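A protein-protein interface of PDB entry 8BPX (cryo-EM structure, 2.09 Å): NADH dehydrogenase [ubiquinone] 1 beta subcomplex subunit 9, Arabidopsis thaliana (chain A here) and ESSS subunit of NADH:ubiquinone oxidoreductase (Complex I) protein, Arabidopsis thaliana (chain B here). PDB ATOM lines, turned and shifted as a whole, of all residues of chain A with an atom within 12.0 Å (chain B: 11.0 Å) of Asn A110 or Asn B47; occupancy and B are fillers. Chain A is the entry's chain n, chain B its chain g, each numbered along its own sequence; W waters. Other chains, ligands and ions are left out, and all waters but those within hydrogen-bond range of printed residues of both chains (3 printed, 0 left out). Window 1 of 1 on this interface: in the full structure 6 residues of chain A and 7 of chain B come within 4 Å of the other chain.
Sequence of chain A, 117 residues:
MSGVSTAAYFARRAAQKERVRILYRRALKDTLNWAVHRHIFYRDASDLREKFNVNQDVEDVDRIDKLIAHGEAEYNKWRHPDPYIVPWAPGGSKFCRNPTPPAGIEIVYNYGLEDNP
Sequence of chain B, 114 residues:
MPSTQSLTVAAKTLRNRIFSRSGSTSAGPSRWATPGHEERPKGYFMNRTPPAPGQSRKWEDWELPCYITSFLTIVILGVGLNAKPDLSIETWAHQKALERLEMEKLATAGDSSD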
ATOM      1  N   ILE A 105     -16.604  16.328  13.277  1.00  0.00           N
ATOM      2  CA  ILE A 105     -15.291  16.474  13.889  1.00  0.00           C
ATOM      3  C   ILE A 105     -15.490  16.709  15.375  1.00  0.00           C
ATOM      4  O   ILE A 105     -16.236  17.606  15.776  1.00  0.00           O
ATOM      5  CB  ILE A 105     -14.502  17.631  13.250  1.00  0.00           C
ATOM      6  CG1 ILE A 105     -14.229  17.348  11.772  1.00  0.00           C
ATOM      7  CG2 ILE A 105     -13.202  17.873  14.007  1.00  0.00           C
ATOM      8  CD1 ILE A 105     -13.717  15.956  11.482  1.00  0.00           C
ATOM      9  N   GLU A 106     -14.859  15.855  16.170  1.00  0.00           N
ATOM     10  CA  GLU A 106     -14.897  15.957  17.643  1.00  0.00           C
ATOM     11  C   GLU A 106     -13.510  16.340  18.204  1.00  0.00           C
ATOM     12  O   GLU A 106     -12.528  15.819  17.710  1.00  0.00           O
ATOM     13  CB  GLU A 106     -15.454  14.646  18.177  1.00  0.00           C
ATOM     14  CG  GLU A 106     -16.821  14.323  17.640  1.00  0.00           C
ATOM     15  CD  GLU A 106     -17.176  12.853  17.612  1.00  0.00           C
ATOM     16  OE1 GLU A 106     -16.932  12.179  18.611  1.00  0.00           O
ATOM     17  OE2 GLU A 106     -17.721  12.398  16.585  1.00  0.00           O
ATOM     18  N   ILE A 107     -13.430  17.232  19.159  1.00  0.00           N
ATOM     19  CA  ILE A 107     -12.181  17.609  19.806  1.00  0.00           C
ATOM     20  C   ILE A 107     -12.201  17.039  21.215  1.00  0.00           C
ATOM     21  O   ILE A 107     -13.167  17.246  21.957  1.00  0.00           O
ATOM     22  CB  ILE A 107     -12.006  19.139  19.833  1.00  0.00           C
ATOM     23  CG1 ILE A 107     -11.981  19.720  18.413  1.00  0.00           C
ATOM     24  CG2 ILE A 107     -10.749  19.521  20.588  1.00  0.00           C
ATOM     25  CD1 ILE A 107     -10.968  19.104  17.487  1.00  0.00           C
ATOM     26  N   VAL A 108     -11.173  16.326  21.602  1.00  0.00           N
ATOM     27  CA  VAL A 108     -11.149  15.641  22.931  1.00  0.00           C
ATOM     28  C   VAL A 108     -10.304  16.472  23.884  1.00  0.00           C
ATOM     29  O   VAL A 108      -9.249  16.981  23.505  1.00  0.00           O
ATOM     30  CB  VAL A 108     -10.632  14.175  22.885  1.00  0.00           C
ATOM     31  CG1 VAL A 108     -10.696  13.423  24.192  1.00  0.00           C
ATOM     32  CG2 VAL A 108     -11.135  13.371  21.718  1.00  0.00           C
ATOM     33  N   TYR A 109     -10.753  16.543  25.088  1.00  0.00           N
ATOM     34  CA  TYR A 109     -10.101  17.251  26.176  1.00  0.00           C
ATOM     35  C   TYR A 109      -9.557  16.247  27.184  1.00  0.00           C
ATOM     36  O   TYR A 109     -10.044  15.117  27.277  1.00  0.00           O
ATOM     37  CB  TYR A 109     -11.081  18.207  26.861  1.00  0.00           C
ATOM     38  CG  TYR A 109     -11.425  19.420  26.034  1.00  0.00           C
ATOM     39  CD1 TYR A 109     -10.540  19.917  25.089  1.00  0.00           C
ATOM     40  CD2 TYR A 109     -12.658  20.040  26.167  1.00  0.00           C
ATOM     41  CE1 TYR A 109     -10.861  21.022  24.327  1.00  0.00           C
ATOM     42  CE2 TYR A 109     -12.989  21.135  25.412  1.00  0.00           C
ATOM     43  CZ  TYR A 109     -12.089  21.623  24.492  1.00  0.00           C
ATOM     44  OH  TYR A 109     -12.425  22.720  23.739  1.00  0.00           O
ATOM     45  N   ASN A 110      -8.528  16.669  27.920  1.00  0.00           N
ATOM     46  CA  ASN A 110      -7.950  15.889  29.016  1.00  0.00           C
ATOM     47  C   ASN A 110      -7.428  14.533  28.538  1.00  0.00           C
ATOM     48  O   ASN A 110      -7.636  13.498  29.172  1.00  0.00           O
ATOM     49  CB  ASN A 110      -8.961  15.719  30.155  1.00  0.00           C
ATOM     50  CG  ASN A 110      -9.649  17.020  30.515  1.00  0.00           C
ATOM     51  OD1 ASN A 110      -8.997  18.021  30.802  1.00  0.00           O
ATOM     52  ND2 ASN A 110     -10.969  17.013  30.493  1.00  0.00           N
ATOM     53  N   TYR A 111      -6.730  14.549  27.412  1.00  0.00           N
ATOM     54  CA  TYR A 111      -6.089  13.361  26.875  1.00  0.00           C
ATOM     55  C   TYR A 111      -4.730  13.133  27.530  1.00  0.00           C
ATOM     56  O   TYR A 111      -4.048  14.073  27.940  1.00  0.00           O
ATOM     57  CB  TYR A 111      -5.921  13.483  25.361  1.00  0.00           C
ATOM     58  CG  TYR A 111      -5.304  12.268  24.709  1.00  0.00           C
ATOM     59  CD1 TYR A 111      -6.044  11.111  24.506  1.00  0.00           C
ATOM     60  CD2 TYR A 111      -3.975  12.274  24.310  1.00  0.00           C
ATOM     61  CE1 TYR A 111      -5.482  10.000  23.919  1.00  0.00           C
ATOM     62  CE2 TYR A 111      -3.404  11.170  23.724  1.00  0.00           C
ATOM     63  CZ  TYR A 111      -4.164  10.032  23.529  1.00  0.00           C
ATOM     64  OH  TYR A 111      -3.599   8.924  22.946  1.00  0.00           O
ATOM     65  N   GLY A 112      -4.349  11.864  27.629  1.00  0.00           N
ATOM     66  CA  GLY A 112      -3.024  11.493  28.088  1.00  0.00           C
ATOM     67  C   GLY A 112      -2.702  11.822  29.530  1.00  0.00           C
ATOM     68  O   GLY A 112      -1.546  12.113  29.841  1.00  0.00           O
ATOM     69  N   LEU A 113      -3.689  11.778  30.418  1.00  0.00           N
ATOM     70  CA  LEU A 113      -3.445  12.035  31.829  1.00  0.00           C
ATOM     71  C   LEU A 113      -2.679  10.877  32.461  1.00  0.00           C
ATOM     72  O   LEU A 113      -2.746   9.736  32.001  1.00  0.00           O
ATOM     73  CB  LEU A 113      -4.768  12.259  32.562  1.00  0.00           C
ATOM     74  CG  LEU A 113      -5.582  13.439  32.024  1.00  0.00           C
ATOM     75  CD1 LEU A 113      -6.982  13.463  32.601  1.00  0.00           C
ATOM     76  CD2 LEU A 113      -4.860  14.735  32.319  1.00  0.00           C
ATOM     77  N   GLU A 114      -1.932  11.185  33.522  1.00  0.00           N
ATOM     78  CA  GLU A 114      -1.119  10.156  34.162  1.00  0.00           C
ATOM     79  C   GLU A 114      -1.977   9.064  34.788  1.00  0.00           C
ATOM     80  O   GLU A 114      -1.525   7.921  34.915  1.00  0.00           O
ATOM     81  CB  GLU A 114      -0.193  10.776  35.209  1.00  0.00           C
ATOM     82  CG  GLU A 114      -0.849  11.757  36.152  1.00  0.00           C
ATOM     83  CD  GLU A 114       0.049  12.110  37.326  1.00  0.00           C
ATOM     84  OE1 GLU A 114       1.278  11.964  37.194  1.00  0.00           O
ATOM     85  OE2 GLU A 114      -0.465  12.553  38.370  1.00  0.00           O
ATOM     86  N   ASP A 115      -3.204   9.383  35.181  1.00  0.00           N
ATOM     87  CA  ASP A 115      -4.092   8.394  35.773  1.00  0.00           C
ATOM     88  C   ASP A 115      -4.791   7.564  34.703  1.00  0.00           C
ATOM     89  O   ASP A 115      -5.399   6.535  35.000  1.00  0.00           O
ATOM     90  CB  ASP A 115      -5.126   9.069  36.672  1.00  0.00           C
ATOM     91  CG  ASP A 115      -4.519   9.616  37.947  1.00  0.00           C
ATOM     92  OD1 ASP A 115      -3.376   9.233  38.273  1.00  0.00           O
ATOM     93  OD2 ASP A 115      -5.183  10.429  38.624  1.00  0.00           O
ATOM     94  N   LYS B  42     -11.591  30.694  22.323  1.00  0.00           N
ATOM     95  CA  LYS B  42     -12.024  29.371  21.806  1.00  0.00           C
ATOM     96  C   LYS B  42     -10.956  28.339  22.178  1.00  0.00           C
ATOM     97  O   LYS B  42      -9.755  28.655  22.055  1.00  0.00           O
ATOM     98  CB  LYS B  42     -12.282  29.445  20.296  1.00  0.00           C
ATOM     99  CG  LYS B  42     -11.168  30.049  19.452  1.00  0.00           C
ATOM    100  CD  LYS B  42     -11.316  29.790  17.968  1.00  0.00           C
ATOM    101  CE  LYS B  42     -12.348  30.663  17.288  1.00  0.00           C
ATOM    102  NZ  LYS B  42     -11.906  32.077  17.214  1.00  0.00           N
ATOM    103  N   GLY B  43     -11.380  27.160  22.628  1.00  0.00           N
ATOM    104  CA  GLY B  43     -10.476  26.116  23.062  1.00  0.00           C
ATOM    105  C   GLY B  43      -9.989  26.309  24.487  1.00  0.00           C
ATOM    106  O   GLY B  43     -10.324  27.265  25.184  1.00  0.00           O
ATOM    107  N   TYR B  44      -9.170  25.361  24.923  1.00  0.00           N
ATOM    108  CA  TYR B  44      -8.509  25.433  26.216  1.00  0.00           C
ATOM    109  C   TYR B  44      -7.030  25.198  25.995  1.00  0.00           C
ATOM    110  O   TYR B  44      -6.653  24.289  25.250  1.00  0.00           O
ATOM    111  CB  TYR B  44      -9.077  24.401  27.192  1.00  0.00           C
ATOM    112  CG  TYR B  44     -10.436  24.789  27.701  1.00  0.00           C
ATOM    113  CD1 TYR B  44     -10.626  25.986  28.370  1.00  0.00           C
ATOM    114  CD2 TYR B  44     -11.537  23.974  27.486  1.00  0.00           C
ATOM    115  CE1 TYR B  44     -11.864  26.357  28.818  1.00  0.00           C
ATOM    116  CE2 TYR B  44     -12.786  24.336  27.940  1.00  0.00           C
ATOM    117  CZ  TYR B  44     -12.942  25.528  28.605  1.00  0.00           C
ATOM    118  OH  TYR B  44     -14.183  25.903  29.065  1.00  0.00           O
ATOM    119  N   PHE B  45      -6.199  26.016  26.630  1.00  0.00           N
ATOM    120  CA  PHE B  45      -4.762  25.879  26.466  1.00  0.00           C
ATOM    121  C   PHE B  45      -4.307  24.491  26.897  1.00  0.00           C
ATOM    122  O   PHE B  45      -4.540  24.078  28.038  1.00  0.00           O
ATOM    123  CB  PHE B  45      -4.034  26.953  27.266  1.00  0.00           C
ATOM    124  CG  PHE B  45      -2.548  26.879  27.138  1.00  0.00           C
ATOM    125  CD1 PHE B  45      -1.744  26.760  28.258  1.00  0.00           C
ATOM    126  CD2 PHE B  45      -1.955  26.890  25.890  1.00  0.00           C
ATOM    127  CE1 PHE B  45      -0.375  26.679  28.134  1.00  0.00           C
ATOM    128  CE2 PHE B  45      -0.584  26.807  25.759  1.00  0.00           C
ATOM    129  CZ  PHE B  45       0.208  26.700  26.884  1.00  0.00           C
ATOM    130  N   MET B  46      -3.660  23.777  25.979  1.00  0.00           N
ATOM    131  CA  MET B  46      -3.215  22.398  26.177  1.00  0.00           C
ATOM    132  C   MET B  46      -4.372  21.441  26.459  1.00  0.00           C
ATOM    133  O   MET B  46      -4.178  20.393  27.078  1.00  0.00           O
ATOM    134  CB  MET B  46      -2.138  22.324  27.269  1.00  0.00           C
ATOM    135  CG  MET B  46      -0.862  23.057  26.849  1.00  0.00           C
ATOM    136  SD  MET B  46       0.392  23.373  28.104  1.00  0.00           S
ATOM    137  CE  MET B  46      -0.543  23.135  29.599  1.00  0.00           C
ATOM    138  N   ASN B  47      -5.572  21.798  25.994  1.00  0.00           N
ATOM    139  CA  ASN B  47      -6.741  20.910  25.957  1.00  0.00           C
ATOM    140  C   ASN B  47      -7.093  20.337  27.327  1.00  0.00           C
ATOM    141  O   ASN B  47      -7.576  19.210  27.440  1.00  0.00           O
ATOM    142  CB  ASN B  47      -6.548  19.776  24.943  1.00  0.00           C
ATOM    143  CG  ASN B  47      -6.712  20.233  23.506  1.00  0.00           C
ATOM    144  OD1 ASN B  47      -6.118  21.226  23.092  1.00  0.00           O
ATOM    145  ND2 ASN B  47      -7.533  19.522  22.742  1.00  0.00           N
ATOM    146  N   ARG B  48      -6.869  21.113  28.379  1.00  0.00           N
ATOM    147  CA  ARG B  48      -7.284  20.722  29.720  1.00  0.00           C
ATOM    148  C   ARG B  48      -8.475  21.571  30.138  1.00  0.00           C
ATOM    149  O   ARG B  48      -8.438  22.797  30.030  1.00  0.00           O
ATOM    150  CB  ARG B  48      -6.150  20.852  30.740  1.00  0.00           C
ATOM    151  CG  ARG B  48      -5.389  22.158  30.705  1.00  0.00           C
ATOM    152  CD  ARG B  48      -4.563  22.333  31.969  1.00  0.00           C
ATOM    153  NE  ARG B  48      -3.327  21.560  31.960  1.00  0.00           N
ATOM    154  CZ  ARG B  48      -2.140  22.049  32.286  1.00  0.00           C
ATOM    155  NH1 ARG B  48      -1.984  23.320  32.623  1.00  0.00           N
ATOM    156  NH2 ARG B  48      -1.080  21.250  32.256  1.00  0.00           N
ATOM    157  N   THR B  49      -9.530  20.917  30.598  1.00  0.00           N
ATOM    158  CA  THR B  49     -10.696  21.642  31.054  1.00  0.00           C
ATOM    159  C   THR B  49     -10.365  22.400  32.339  1.00  0.00           C
ATOM    160  O   THR B  49      -9.564  21.938  33.151  1.00  0.00           O
ATOM    161  CB  THR B  49     -11.866  20.696  31.278  1.00  0.00           C
ATOM    162  OG1 THR B  49     -11.494  19.683  32.219  1.00  0.00           O
ATOM    163  CG2 THR B  49     -12.257  20.041  29.970  1.00  0.00           C
ATOM    164  N   PRO B  50     -10.944  23.586  32.527  1.00  0.00           N
ATOM    165  CA  PRO B  50     -10.604  24.387  33.704  1.00  0.00           C
ATOM    166  C   PRO B  50     -11.081  23.719  34.980  1.00  0.00           C
ATOM    167  O   PRO B  50     -12.007  22.893  34.958  1.00  0.00           O
ATOM    168  CB  PRO B  50     -11.359  25.694  33.426  1.00  0.00           C
ATOM    169  CG  PRO B  50     -12.512  24.936  32.743  1.00  0.00           C
ATOM    170  CD  PRO B  50     -11.746  24.488  31.655  1.00  0.00           C
ATOM    171  N   PRO B  51     -10.451  24.013  36.110  1.00  0.00           N
ATOM    172  CA  PRO B  51     -10.928  23.459  37.381  1.00  0.00           C
ATOM    173  C   PRO B  51     -12.249  24.096  37.781  1.00  0.00           C
ATOM    174  O   PRO B  51     -12.656  25.139  37.265  1.00  0.00           O
ATOM    175  CB  PRO B  51      -9.805  23.794  38.361  1.00  0.00           C
ATOM    176  CG  PRO B  51      -9.143  24.985  37.772  1.00  0.00           C
ATOM    177  CD  PRO B  51      -9.261  24.861  36.286  1.00  0.00           C
ATOM    178  N   ALA B  52     -12.925  23.435  38.715  1.00  0.00           N
ATOM    179  CA  ALA B  52     -14.198  23.933  39.211  1.00  0.00           C
ATOM    180  C   ALA B  52     -14.003  25.316  39.835  1.00  0.00           C
ATOM    181  O   ALA B  52     -12.928  25.614  40.365  1.00  0.00           O
ATOM    182  CB  ALA B  52     -14.780  22.962  40.235  1.00  0.00           C
ATOM    183  N   ARG B  57      -6.014  23.797  39.683  1.00  0.00           N
ATOM    184  CA  ARG B  57      -5.667  22.605  38.925  1.00  0.00           C
ATOM    185  C   ARG B  57      -4.723  21.730  39.741  1.00  0.00           C
ATOM    186  O   ARG B  57      -3.822  22.223  40.420  1.00  0.00           O
ATOM    187  CB  ARG B  57      -5.033  22.989  37.589  1.00  0.00           C
ATOM    188  CG  ARG B  57      -4.487  21.812  36.810  1.00  0.00           C
ATOM    189  CD  ARG B  57      -3.757  22.245  35.557  1.00  0.00           C
ATOM    190  NE  ARG B  57      -2.465  22.843  35.859  1.00  0.00           N
ATOM    191  CZ  ARG B  57      -1.314  22.187  35.845  1.00  0.00           C
ATOM    192  NH1 ARG B  57      -1.263  20.888  35.613  1.00  0.00           N
ATOM    193  NH2 ARG B  57      -0.186  22.850  36.084  1.00  0.00           N
ATOM    194  N   LYS B  58      -4.962  20.423  39.704  1.00  0.00           N
ATOM    195  CA  LYS B  58      -4.106  19.475  40.400  1.00  0.00           C
ATOM    196  C   LYS B  58      -2.887  19.198  39.526  1.00  0.00           C
ATOM    197  O   LYS B  58      -3.026  18.871  38.343  1.00  0.00           O
ATOM    198  CB  LYS B  58      -4.913  18.210  40.721  1.00  0.00           C
ATOM    199  CG  LYS B  58      -4.256  17.071  41.521  1.00  0.00           C
ATOM    200  CD  LYS B  58      -5.129  15.865  41.846  1.00  0.00           C
ATOM    201  CE  LYS B  58      -4.364  14.795  42.618  1.00  0.00           C
ATOM    202  NZ  LYS B  58      -5.208  13.613  42.939  1.00  0.00           N
ATOM    203  N   GLU B  60       0.172  17.246  37.992  1.00  0.00           N
ATOM    204  CA  GLU B  60       0.596  15.867  37.807  1.00  0.00           C
ATOM    205  C   GLU B  60       1.951  15.633  38.471  1.00  0.00           C
ATOM    206  O   GLU B  60       2.711  16.563  38.744  1.00  0.00           O
ATOM    207  CB  GLU B  60       0.645  15.507  36.325  1.00  0.00           C
ATOM    208  CG  GLU B  60      -0.652  15.765  35.587  1.00  0.00           C
ATOM    209  CD  GLU B  60      -0.839  14.852  34.390  1.00  0.00           C
ATOM    210  OE1 GLU B  60       0.054  14.822  33.519  1.00  0.00           O
ATOM    211  OE2 GLU B  60      -1.883  14.171  34.314  1.00  0.00           O
HETATM  212  O   HOH W   1     -13.248  25.289  24.373  1.00  0.00           O
HETATM  213  O   HOH W   2       0.353  13.155  31.494  1.00  0.00           O
HETATM  214  O   HOH W   3      -4.926  17.025  27.517  1.00  0.00           O
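ND2 of Asn B47 sits at hydrogen-bond distance from O of Val A108, 3.2 Å away.
The backbone carbonyl oxygen (O) of Asn B47 sits at hydrogen-bond distance from the backbone NH (N) of Asn A110, at 2.8 Å.
N of Thr B49 lies within hydrogen-bond range of OD1 of Asn A110, at 3.0 Å.
N of Glu A114 sits at hydrogen-bond distance from OE2 of Glu B60, at 3.1 Å.
Among the printed residues, pairs that only touch across the chains: Asn A110 with Arg B48 (3.4 Å), Tyr A109 with Asn B47 (3.4 Å), Leu A113 with Glu B60 (3.6 Å), Tyr A109 with Thr B49 (3.8 Å), Tyr A109 with Tyr B44 (3.8 Å), Ile A107 with Asn B47 (3.9 Å) and Tyr A109 with Gly B43 (3.97 Å).
Of the printed residues of chain B, Ile A107 touches Asn B47 (3.9 Å).
Tyr A109 touches just these residues of chain B: Gly B43 (3.97 Å), Tyr B44 (3.8 Å), Asn B47 (3.4 Å) and Thr B49 (3.8 Å).
Asn A110 touches just these residues of chain B: Asn B47 (2.8 Å), Arg B48 (3.4 Å) and Thr B49 (3.0 Å).
Leu A113 touches just one residue of chain B: Glu B60.
Of the printed residues of chain B, Glu A114 touches Glu B60.
Of chain A, only Tyr A109 comes within 4 Å of Gly B43.
No residue of chain A comes within 4 Å of Met B46.
Arg B48 touches just one residue of chain A: Asn A110 (3.4 Å).
Of chain A, only Tyr A109 and Asn A110 come within 4 Å of Thr B49.
The nearest residue of chain A that does not touch Asn B47 is Tyr A111 (4.7 Å).
The nearest printed residue of chain A that does not touch Glu B60 is Gly A112 (4.8 Å).
Hydrophobic or aromatic side chains of chain A within 4 Å of the printed part of chain B: Ile A107, Tyr A109 and Leu A113.
Water W2 bridges the side-chain carboxylate of Glu B60 (2.6 Å) and the backbone carbonyl oxygen of Gly A112 (2.7 Å).
Water W1 bridges the side-chain hydroxyl of Tyr A109 (2.8 Å) and the backbone NH of Gly B43 (3.2 Å).
Water W3 lies within hydrogen-bond range of N of Tyr A111 (3.1 Å), O of Asn B47 (3.4 Å) and O of Met B46 (3.5 Å).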
